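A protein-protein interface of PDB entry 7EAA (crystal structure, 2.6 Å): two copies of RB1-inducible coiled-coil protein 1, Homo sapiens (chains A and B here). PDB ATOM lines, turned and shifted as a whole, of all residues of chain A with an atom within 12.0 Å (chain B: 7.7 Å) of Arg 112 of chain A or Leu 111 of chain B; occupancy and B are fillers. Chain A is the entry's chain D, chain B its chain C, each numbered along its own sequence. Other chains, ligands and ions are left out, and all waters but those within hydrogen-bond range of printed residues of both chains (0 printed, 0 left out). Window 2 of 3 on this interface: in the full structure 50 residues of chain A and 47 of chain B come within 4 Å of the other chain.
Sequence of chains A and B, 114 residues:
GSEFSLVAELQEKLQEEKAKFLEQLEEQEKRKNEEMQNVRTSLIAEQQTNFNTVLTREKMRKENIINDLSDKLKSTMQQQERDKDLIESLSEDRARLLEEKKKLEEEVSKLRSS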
ATOM      1  N   LYS A 101      -6.863 -17.919  11.191  1.00  0.00           N
ATOM      2  CA  LYS A 101      -6.266 -18.817  10.221  1.00  0.00           C
ATOM      3  C   LYS A 101      -6.788 -20.225  10.417  1.00  0.00           C
ATOM      4  O   LYS A 101      -6.975 -20.961   9.444  1.00  0.00           O
ATOM      5  CB  LYS A 101      -4.749 -18.769  10.331  1.00  0.00           C
ATOM      6  CG  LYS A 101      -4.021 -19.717   9.395  1.00  0.00           C
ATOM      7  CD  LYS A 101      -2.528 -19.724   9.699  1.00  0.00           C
ATOM      8  CE  LYS A 101      -1.916 -21.103   9.492  1.00  0.00           C
ATOM      9  NZ  LYS A 101      -1.475 -21.344   8.080  1.00  0.00           N
ATOM     10  N   LYS A 102      -7.089 -20.595  11.656  1.00  0.00           N
ATOM     11  CA  LYS A 102      -7.626 -21.921  11.902  1.00  0.00           C
ATOM     12  C   LYS A 102      -9.039 -22.043  11.337  1.00  0.00           C
ATOM     13  O   LYS A 102      -9.353 -23.016  10.639  1.00  0.00           O
ATOM     14  CB  LYS A 102      -7.597 -22.219  13.398  1.00  0.00           C
ATOM     15  CG  LYS A 102      -7.679 -23.696  13.712  1.00  0.00           C
ATOM     16  CD  LYS A 102      -7.781 -23.963  15.205  1.00  0.00           C
ATOM     17  CE  LYS A 102      -9.251 -24.011  15.654  1.00  0.00           C
ATOM     18  NZ  LYS A 102      -9.776 -25.381  15.972  1.00  0.00           N
ATOM     19  N   LYS A 103      -9.900 -21.042  11.595  1.00  0.00           N
ATOM     20  CA  LYS A 103     -11.275 -21.093  11.094  1.00  0.00           C
ATOM     21  C   LYS A 103     -11.329 -21.021   9.573  1.00  0.00           C
ATOM     22  O   LYS A 103     -12.266 -21.557   8.968  1.00  0.00           O
ATOM     23  CB  LYS A 103     -12.110 -19.965  11.691  1.00  0.00           C
ATOM     24  CG  LYS A 103     -12.393 -20.141  13.148  1.00  0.00           C
ATOM     25  CD  LYS A 103     -13.111 -18.950  13.739  1.00  0.00           C
ATOM     26  CE  LYS A 103     -13.382 -19.169  15.235  1.00  0.00           C
ATOM     27  NZ  LYS A 103     -13.702 -17.907  15.952  1.00  0.00           N
ATOM     28  N   LEU A 104     -10.347 -20.367   8.940  1.00  0.00           N
ATOM     29  CA  LEU A 104     -10.279 -20.375   7.480  1.00  0.00           C
ATOM     30  C   LEU A 104      -9.878 -21.746   6.957  1.00  0.00           C
ATOM     31  O   LEU A 104     -10.359 -22.179   5.907  1.00  0.00           O
ATOM     32  CB  LEU A 104      -9.296 -19.317   6.985  1.00  0.00           C
ATOM     33  CG  LEU A 104      -9.830 -17.889   6.898  1.00  0.00           C
ATOM     34  CD1 LEU A 104      -8.679 -16.937   6.654  1.00  0.00           C
ATOM     35  CD2 LEU A 104     -10.843 -17.765   5.782  1.00  0.00           C
ATOM     36  N   GLU A 105      -8.980 -22.434   7.668  1.00  0.00           N
ATOM     37  CA  GLU A 105      -8.586 -23.785   7.279  1.00  0.00           C
ATOM     38  C   GLU A 105      -9.741 -24.764   7.415  1.00  0.00           C
ATOM     39  O   GLU A 105      -9.854 -25.706   6.619  1.00  0.00           O
ATOM     40  CB  GLU A 105      -7.404 -24.254   8.118  1.00  0.00           C
ATOM     41  CG  GLU A 105      -6.061 -23.952   7.510  1.00  0.00           C
ATOM     42  CD  GLU A 105      -5.004 -23.705   8.565  1.00  0.00           C
ATOM     43  OE1 GLU A 105      -3.888 -23.279   8.184  1.00  0.00           O
ATOM     44  OE2 GLU A 105      -5.289 -23.931   9.770  1.00  0.00           O
ATOM     45  N   GLU A 106     -10.607 -24.566   8.413  1.00  0.00           N
ATOM     46  CA  GLU A 106     -11.792 -25.401   8.511  1.00  0.00           C
ATOM     47  C   GLU A 106     -12.772 -25.093   7.381  1.00  0.00           C
ATOM     48  O   GLU A 106     -13.385 -26.007   6.816  1.00  0.00           O
ATOM     49  CB  GLU A 106     -12.448 -25.225   9.881  1.00  0.00           C
ATOM     50  CG  GLU A 106     -11.703 -25.960  10.995  1.00  0.00           C
ATOM     51  CD  GLU A 106     -11.570 -25.145  12.286  1.00  0.00           C
ATOM     52  OE1 GLU A 106     -10.689 -25.478  13.119  1.00  0.00           O
ATOM     53  OE2 GLU A 106     -12.349 -24.178  12.469  1.00  0.00           O
ATOM     54  N   GLU A 107     -12.909 -23.815   7.022  1.00  0.00           N
ATOM     55  CA  GLU A 107     -13.796 -23.436   5.927  1.00  0.00           C
ATOM     56  C   GLU A 107     -13.305 -24.006   4.603  1.00  0.00           C
ATOM     57  O   GLU A 107     -14.097 -24.523   3.807  1.00  0.00           O
ATOM     58  CB  GLU A 107     -13.903 -21.912   5.866  1.00  0.00           C
ATOM     59  CG  GLU A 107     -14.902 -21.358   4.859  1.00  0.00           C
ATOM     60  CD  GLU A 107     -15.126 -19.849   5.022  1.00  0.00           C
ATOM     61  OE1 GLU A 107     -14.482 -19.223   5.908  1.00  0.00           O
ATOM     62  OE2 GLU A 107     -15.960 -19.293   4.266  1.00  0.00           O
ATOM     63  N   VAL A 108     -11.998 -23.936   4.357  1.00  0.00           N
ATOM     64  CA  VAL A 108     -11.433 -24.539   3.153  1.00  0.00           C
ATOM     65  C   VAL A 108     -11.699 -26.037   3.146  1.00  0.00           C
ATOM     66  O   VAL A 108     -12.159 -26.592   2.147  1.00  0.00           O
ATOM     67  CB  VAL A 108      -9.927 -24.228   3.051  1.00  0.00           C
ATOM     68  CG1 VAL A 108      -9.264 -25.080   1.999  1.00  0.00           C
ATOM     69  CG2 VAL A 108      -9.705 -22.767   2.706  1.00  0.00           C
ATOM     70  N   SER A 109     -11.424 -26.712   4.269  1.00  0.00           N
ATOM     71  CA  SER A 109     -11.624 -28.161   4.344  1.00  0.00           C
ATOM     72  C   SER A 109     -13.059 -28.550   4.022  1.00  0.00           C
ATOM     73  O   SER A 109     -13.301 -29.440   3.199  1.00  0.00           O
ATOM     74  CB  SER A 109     -11.243 -28.682   5.728  1.00  0.00           C
ATOM     75  OG  SER A 109      -9.895 -29.104   5.743  1.00  0.00           O
ATOM     76  N   LYS A 110     -14.030 -27.898   4.668  1.00  0.00           N
ATOM     77  CA  LYS A 110     -15.428 -28.221   4.408  1.00  0.00           C
ATOM     78  C   LYS A 110     -15.793 -27.973   2.948  1.00  0.00           C
ATOM     79  O   LYS A 110     -16.508 -28.773   2.338  1.00  0.00           O
ATOM     80  CB  LYS A 110     -16.348 -27.418   5.330  1.00  0.00           C
ATOM     81  CG  LYS A 110     -16.242 -27.840   6.802  1.00  0.00           C
ATOM     82  CD  LYS A 110     -17.417 -27.347   7.641  1.00  0.00           C
ATOM     83  CE  LYS A 110     -17.034 -26.181   8.549  1.00  0.00           C
ATOM     84  NZ  LYS A 110     -16.782 -24.875   7.826  1.00  0.00           N
ATOM     85  N   LEU A 111     -15.289 -26.883   2.356  1.00  0.00           N
ATOM     86  CA  LEU A 111     -15.618 -26.603   0.961  1.00  0.00           C
ATOM     87  C   LEU A 111     -14.969 -27.614   0.021  1.00  0.00           C
ATOM     88  O   LEU A 111     -15.554 -27.963  -1.010  1.00  0.00           O
ATOM     89  CB  LEU A 111     -15.206 -25.182   0.591  1.00  0.00           C
ATOM     90  CG  LEU A 111     -16.199 -24.044   0.898  1.00  0.00           C
ATOM     91  CD1 LEU A 111     -16.843 -24.122   2.293  1.00  0.00           C
ATOM     92  CD2 LEU A 111     -15.536 -22.684   0.722  1.00  0.00           C
ATOM     93  N   ARG A 112     -13.766 -28.098   0.351  1.00  0.00           N
ATOM     94  CA  ARG A 112     -13.122 -29.091  -0.508  1.00  0.00           C
ATOM     95  C   ARG A 112     -13.866 -30.422  -0.494  1.00  0.00           C
ATOM     96  O   ARG A 112     -13.930 -31.102  -1.525  1.00  0.00           O
ATOM     97  CB  ARG A 112     -11.671 -29.315  -0.095  1.00  0.00           C
ATOM     98  CG  ARG A 112     -10.688 -28.270  -0.551  1.00  0.00           C
ATOM     99  CD  ARG A 112      -9.294 -28.818  -0.413  1.00  0.00           C
ATOM    100  NE  ARG A 112      -8.357 -27.842   0.132  1.00  0.00           N
ATOM    101  CZ  ARG A 112      -7.803 -26.868  -0.587  1.00  0.00           C
ATOM    102  NH1 ARG A 112      -8.115 -26.735  -1.875  1.00  0.00           N
ATOM    103  NH2 ARG A 112      -6.942 -26.028  -0.029  1.00  0.00           N
ATOM    104  N   SER A 113     -14.432 -30.807   0.648  1.00  0.00           N
ATOM    105  CA  SER A 113     -15.110 -32.088   0.810  1.00  0.00           C
ATOM    106  C   SER A 113     -16.632 -31.982   0.700  1.00  0.00           C
ATOM    107  O   SER A 113     -17.330 -32.933   1.068  1.00  0.00           O
ATOM    108  CB  SER A 113     -14.744 -32.699   2.163  1.00  0.00           C
ATOM    109  OG  SER A 113     -13.364 -32.540   2.450  1.00  0.00           O
ATOM    110  N   SER A 114     -17.157 -30.838   0.251  1.00  0.00           N
ATOM    111  CA  SER A 114     -18.594 -30.598   0.092  1.00  0.00           C
ATOM    112  C   SER A 114     -19.220 -31.477  -0.982  1.00  0.00           C
ATOM    113  O   SER A 114     -20.436 -31.417  -1.233  1.00  0.00           O
ATOM    114  CB  SER A 114     -18.864 -29.130  -0.252  1.00  0.00           C
ATOM    115  OG  SER A 114     -19.142 -28.366   0.909  1.00  0.00           O
ATOM    116  OXT SER A 114     -18.516 -32.255  -1.634  1.00  0.00           O
ATOM    117  N   LEU B 104      -5.089 -18.144   2.169  1.00  0.00           N
ATOM    118  CA  LEU B 104      -6.277 -18.933   2.483  1.00  0.00           C
ATOM    119  C   LEU B 104      -7.542 -18.225   2.033  1.00  0.00           C
ATOM    120  O   LEU B 104      -8.462 -18.860   1.513  1.00  0.00           O
ATOM    121  CB  LEU B 104      -6.345 -19.218   3.979  1.00  0.00           C
ATOM    122  CG  LEU B 104      -5.458 -20.338   4.517  1.00  0.00           C
ATOM    123  CD1 LEU B 104      -5.151 -20.042   5.965  1.00  0.00           C
ATOM    124  CD2 LEU B 104      -6.134 -21.710   4.363  1.00  0.00           C
ATOM    125  N   GLU B 105      -7.613 -16.905   2.228  1.00  0.00           N
ATOM    126  CA  GLU B 105      -8.765 -16.161   1.729  1.00  0.00           C
ATOM    127  C   GLU B 105      -8.866 -16.259   0.212  1.00  0.00           C
ATOM    128  O   GLU B 105      -9.971 -16.401  -0.330  1.00  0.00           O
ATOM    129  CB  GLU B 105      -8.706 -14.709   2.199  1.00  0.00           C
ATOM    130  CG  GLU B 105      -9.441 -14.502   3.516  1.00  0.00           C
ATOM    131  CD  GLU B 105      -8.938 -13.318   4.338  1.00  0.00           C
ATOM    132  OE1 GLU B 105      -8.021 -12.595   3.884  1.00  0.00           O
ATOM    133  OE2 GLU B 105      -9.463 -13.123   5.461  1.00  0.00           O
ATOM    134  N   GLU B 106      -7.726 -16.245  -0.492  1.00  0.00           N
ATOM    135  CA  GLU B 106      -7.777 -16.426  -1.943  1.00  0.00           C
ATOM    136  C   GLU B 106      -8.261 -17.820  -2.286  1.00  0.00           C
ATOM    137  O   GLU B 106      -9.026 -18.003  -3.240  1.00  0.00           O
ATOM    138  CB  GLU B 106      -6.413 -16.161  -2.586  1.00  0.00           C
ATOM    139  CG  GLU B 106      -6.068 -14.658  -2.703  1.00  0.00           C
ATOM    140  CD  GLU B 106      -4.569 -14.350  -2.586  1.00  0.00           C
ATOM    141  OE1 GLU B 106      -4.215 -13.193  -2.253  1.00  0.00           O
ATOM    142  OE2 GLU B 106      -3.742 -15.258  -2.831  1.00  0.00           O
ATOM    143  N   GLU B 107      -7.860 -18.818  -1.497  1.00  0.00           N
ATOM    144  CA  GLU B 107      -8.311 -20.173  -1.783  1.00  0.00           C
ATOM    145  C   GLU B 107      -9.796 -20.333  -1.473  1.00  0.00           C
ATOM    146  O   GLU B 107     -10.521 -20.979  -2.237  1.00  0.00           O
ATOM    147  CB  GLU B 107      -7.460 -21.189  -1.020  1.00  0.00           C
ATOM    148  CG  GLU B 107      -7.893 -22.644  -1.185  1.00  0.00           C
ATOM    149  CD  GLU B 107      -7.864 -23.151  -2.639  1.00  0.00           C
ATOM    150  OE1 GLU B 107      -8.392 -24.266  -2.899  1.00  0.00           O
ATOM    151  OE2 GLU B 107      -7.311 -22.446  -3.517  1.00  0.00           O
ATOM    152  N   VAL B 108     -10.287 -19.714  -0.398  1.00  0.00           N
ATOM    153  CA  VAL B 108     -11.718 -19.807  -0.107  1.00  0.00           C
ATOM    154  C   VAL B 108     -12.536 -19.232  -1.257  1.00  0.00           C
ATOM    155  O   VAL B 108     -13.471 -19.867  -1.754  1.00  0.00           O
ATOM    156  CB  VAL B 108     -12.070 -19.096   1.209  1.00  0.00           C
ATOM    157  CG1 VAL B 108     -13.574 -18.944   1.292  1.00  0.00           C
ATOM    158  CG2 VAL B 108     -11.570 -19.875   2.389  1.00  0.00           C
ATOM    159  N   SER B 109     -12.207 -18.017  -1.691  1.00  0.00           N
ATOM    160  CA  SER B 109     -13.073 -17.359  -2.659  1.00  0.00           C
ATOM    161  C   SER B 109     -13.031 -18.070  -4.000  1.00  0.00           C
ATOM    162  O   SER B 109     -14.031 -18.089  -4.724  1.00  0.00           O
ATOM    163  CB  SER B 109     -12.693 -15.879  -2.797  1.00  0.00           C
ATOM    164  OG  SER B 109     -11.763 -15.664  -3.843  1.00  0.00           O
ATOM    165  N   LYS B 110     -11.896 -18.681  -4.333  1.00  0.00           N
ATOM    166  CA  LYS B 110     -11.825 -19.530  -5.520  1.00  0.00           C
ATOM    167  C   LYS B 110     -12.720 -20.765  -5.378  1.00  0.00           C
ATOM    168  O   LYS B 110     -13.327 -21.219  -6.357  1.00  0.00           O
ATOM    169  CB  LYS B 110     -10.362 -19.917  -5.754  1.00  0.00           C
ATOM    170  CG  LYS B 110     -10.070 -20.919  -6.838  1.00  0.00           C
ATOM    171  CD  LYS B 110      -8.559 -21.021  -7.005  1.00  0.00           C
ATOM    172  CE  LYS B 110      -8.130 -22.334  -7.672  1.00  0.00           C
ATOM    173  NZ  LYS B 110      -6.647 -22.569  -7.541  1.00  0.00           N
ATOM    174  N   LEU B 111     -12.827 -21.318  -4.160  1.00  0.00           N
ATOM    175  CA  LEU B 111     -13.665 -22.494  -3.937  1.00  0.00           C
ATOM    176  C   LEU B 111     -15.147 -22.154  -3.882  1.00  0.00           C
ATOM    177  O   LEU B 111     -15.966 -22.987  -4.270  1.00  0.00           O
ATOM    178  CB  LEU B 111     -13.262 -23.209  -2.646  1.00  0.00           C
ATOM    179  CG  LEU B 111     -11.964 -24.018  -2.737  1.00  0.00           C
ATOM    180  CD1 LEU B 111     -11.672 -24.734  -1.431  1.00  0.00           C
ATOM    181  CD2 LEU B 111     -12.021 -25.008  -3.889  1.00  0.00           C
ATOM    182  N   ARG B 112     -15.518 -20.958  -3.409  1.00  0.00           N
ATOM    183  CA  ARG B 112     -16.932 -20.572  -3.402  1.00  0.00           C
ATOM    184  C   ARG B 112     -17.423 -20.237  -4.808  1.00  0.00           C
ATOM    185  O   ARG B 112     -18.522 -20.650  -5.208  1.00  0.00           O
ATOM    186  CB  ARG B 112     -17.154 -19.391  -2.463  1.00  0.00           C
ATOM    187  CG  ARG B 112     -16.642 -19.639  -1.075  1.00  0.00           C
ATOM    188  CD  ARG B 112     -17.139 -18.598  -0.100  1.00  0.00           C
ATOM    189  NE  ARG B 112     -17.397 -19.202   1.199  1.00  0.00           N
ATOM    190  CZ  ARG B 112     -18.457 -19.962   1.457  1.00  0.00           C
ATOM    191  NH1 ARG B 112     -19.353 -20.206   0.502  1.00  0.00           N
ATOM    192  NH2 ARG B 112     -18.618 -20.481   2.668  1.00  0.00           N
ATOM    193  N   SER B 113     -16.622 -19.496  -5.577  1.00  0.00           N
ATOM    194  CA  SER B 113     -16.875 -19.329  -7.003  1.00  0.00           C
ATOM    195  C   SER B 113     -16.622 -20.613  -7.786  1.00  0.00           C
ATOM    196  O   SER B 113     -16.872 -20.644  -8.997  1.00  0.00           O
ATOM    197  CB  SER B 113     -16.004 -18.208  -7.562  1.00  0.00           C
ATOM    198  OG  SER B 113     -14.674 -18.650  -7.792  1.00  0.00           O
ATOM    199  N   SER B 114     -16.128 -21.650  -7.102  1.00  0.00           N
ATOM    200  CA  SER B 114     -15.922 -23.023  -7.591  1.00  0.00           C
ATOM    201  C   SER B 114     -14.759 -23.103  -8.576  1.00  0.00           C
ATOM    202  O   SER B 114     -14.031 -24.104  -8.588  1.00  0.00           O
ATOM    203  CB  SER B 114     -17.212 -23.570  -8.225  1.00  0.00           C
ATOM    204  OG  SER B 114     -18.289 -23.520  -7.295  1.00  0.00           O
ATOM    205  OXT SER B 114     -14.520 -22.166  -9.339  1.00  0.00           O
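The guanidinium group (NH1) of Arg 112 of chain A lies within salt-bridge range of the side-chain carboxylate (OE1) of Glu 107 of chain B (2.7 Å). NH2 of Arg 112 of chain B is in salt-bridge range of OE2 of Glu 107 of chain A, at 3.3 Å.
The side-chain amino group (NZ) of Lys 101 of chain A lies within salt-bridge range of the side-chain carboxylate (OE1) of Glu 105 of chain A (3.1 Å).
CG of Lys 101 of chain A touches CD1 of Leu 104 of chain B (3.6 Å). CG of Glu 105 of chain A touches CD2 of Leu 104 of chain B (3.9 Å). Glu 107 of chain A touches Val 108 of chain B. CG2 of Val 108 of chain A touches CG2 of Val 108 of chain B, 3.5 Å away. Arg 112 of chain B touches Leu 111 of chain A (CG to CD2, 3.7 Å). Arg 112 of chain A touches Leu 111 of chain B.
Of the printed residues of chain B, Lys 101 of chain A touches Leu 104. Of the printed residues of chain B, Glu 105 of chain A touches Leu 104. Of the printed residues of chain B, Glu 107 of chain A touches Val 108 (3.8 Å) and Arg 112 (3.3 Å). Of chain B, only Glu 107 and Leu 111 come within 4 Å of Arg 112 of chain A. Of the printed residues of chain A, Leu 104 of chain B touches Lys 101 (3.6 Å) and Glu 105 (3.9 Å). Val 108 of chain B touches just these residues of chain A: Glu 107 and Val 108. No residue of chain A comes within 4 Å of Lys 110 of chain B. Of chain A, only Arg 112 comes within 4 Å of Leu 111 of chain B. Arg 112 of chain B touches two residues of chain A. No residue of chain A comes within 4 Å of Ser 114 of chain B. The nearest printed residue of chain B that does not touch Leu 111 of chain A is Leu 111 of chain B (4.1 Å).
Hydrophobic or aromatic side chains of chain B that line the printed part of chain A: Leu 104, Val 108 and Leu 111. Of the 14 printed residues of chain A, 6 touch a printed residue of chain B. Printed residues of chain A that touch a printed residue of chain B: Lys 101, Glu 105, Glu 107, Val 108, Leu 111 and Arg 112.
Glu 105 of chain A touches Leu 104 of chain B, but with the chains exchanged Leu 104 of chain A does not touch Glu 105 of chain B (4.04 Å). Glu 107 of chain A touches Val 108 of chain B, but with the chains exchanged Val 108 of chain A does not touch Glu 107 of chain B (4.2 Å). Glu 107 of chain A touches Arg 112 of chain B, and with the chains exchanged Arg 112 of chain A touches Glu 107 of chain B. Leu 111 of chain A touches Arg 112 of chain B, and with the chains exchanged Arg 112 of chain A touches Leu 111 of chain B. Positions printed for both chains: 104, 105, 106, 107, 108, 109, 110, 111, 112, 113 and 114. Of the 8 pairs that touch across the chains among the printed residues, 5 have their exchanged pair printed and touching as well.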
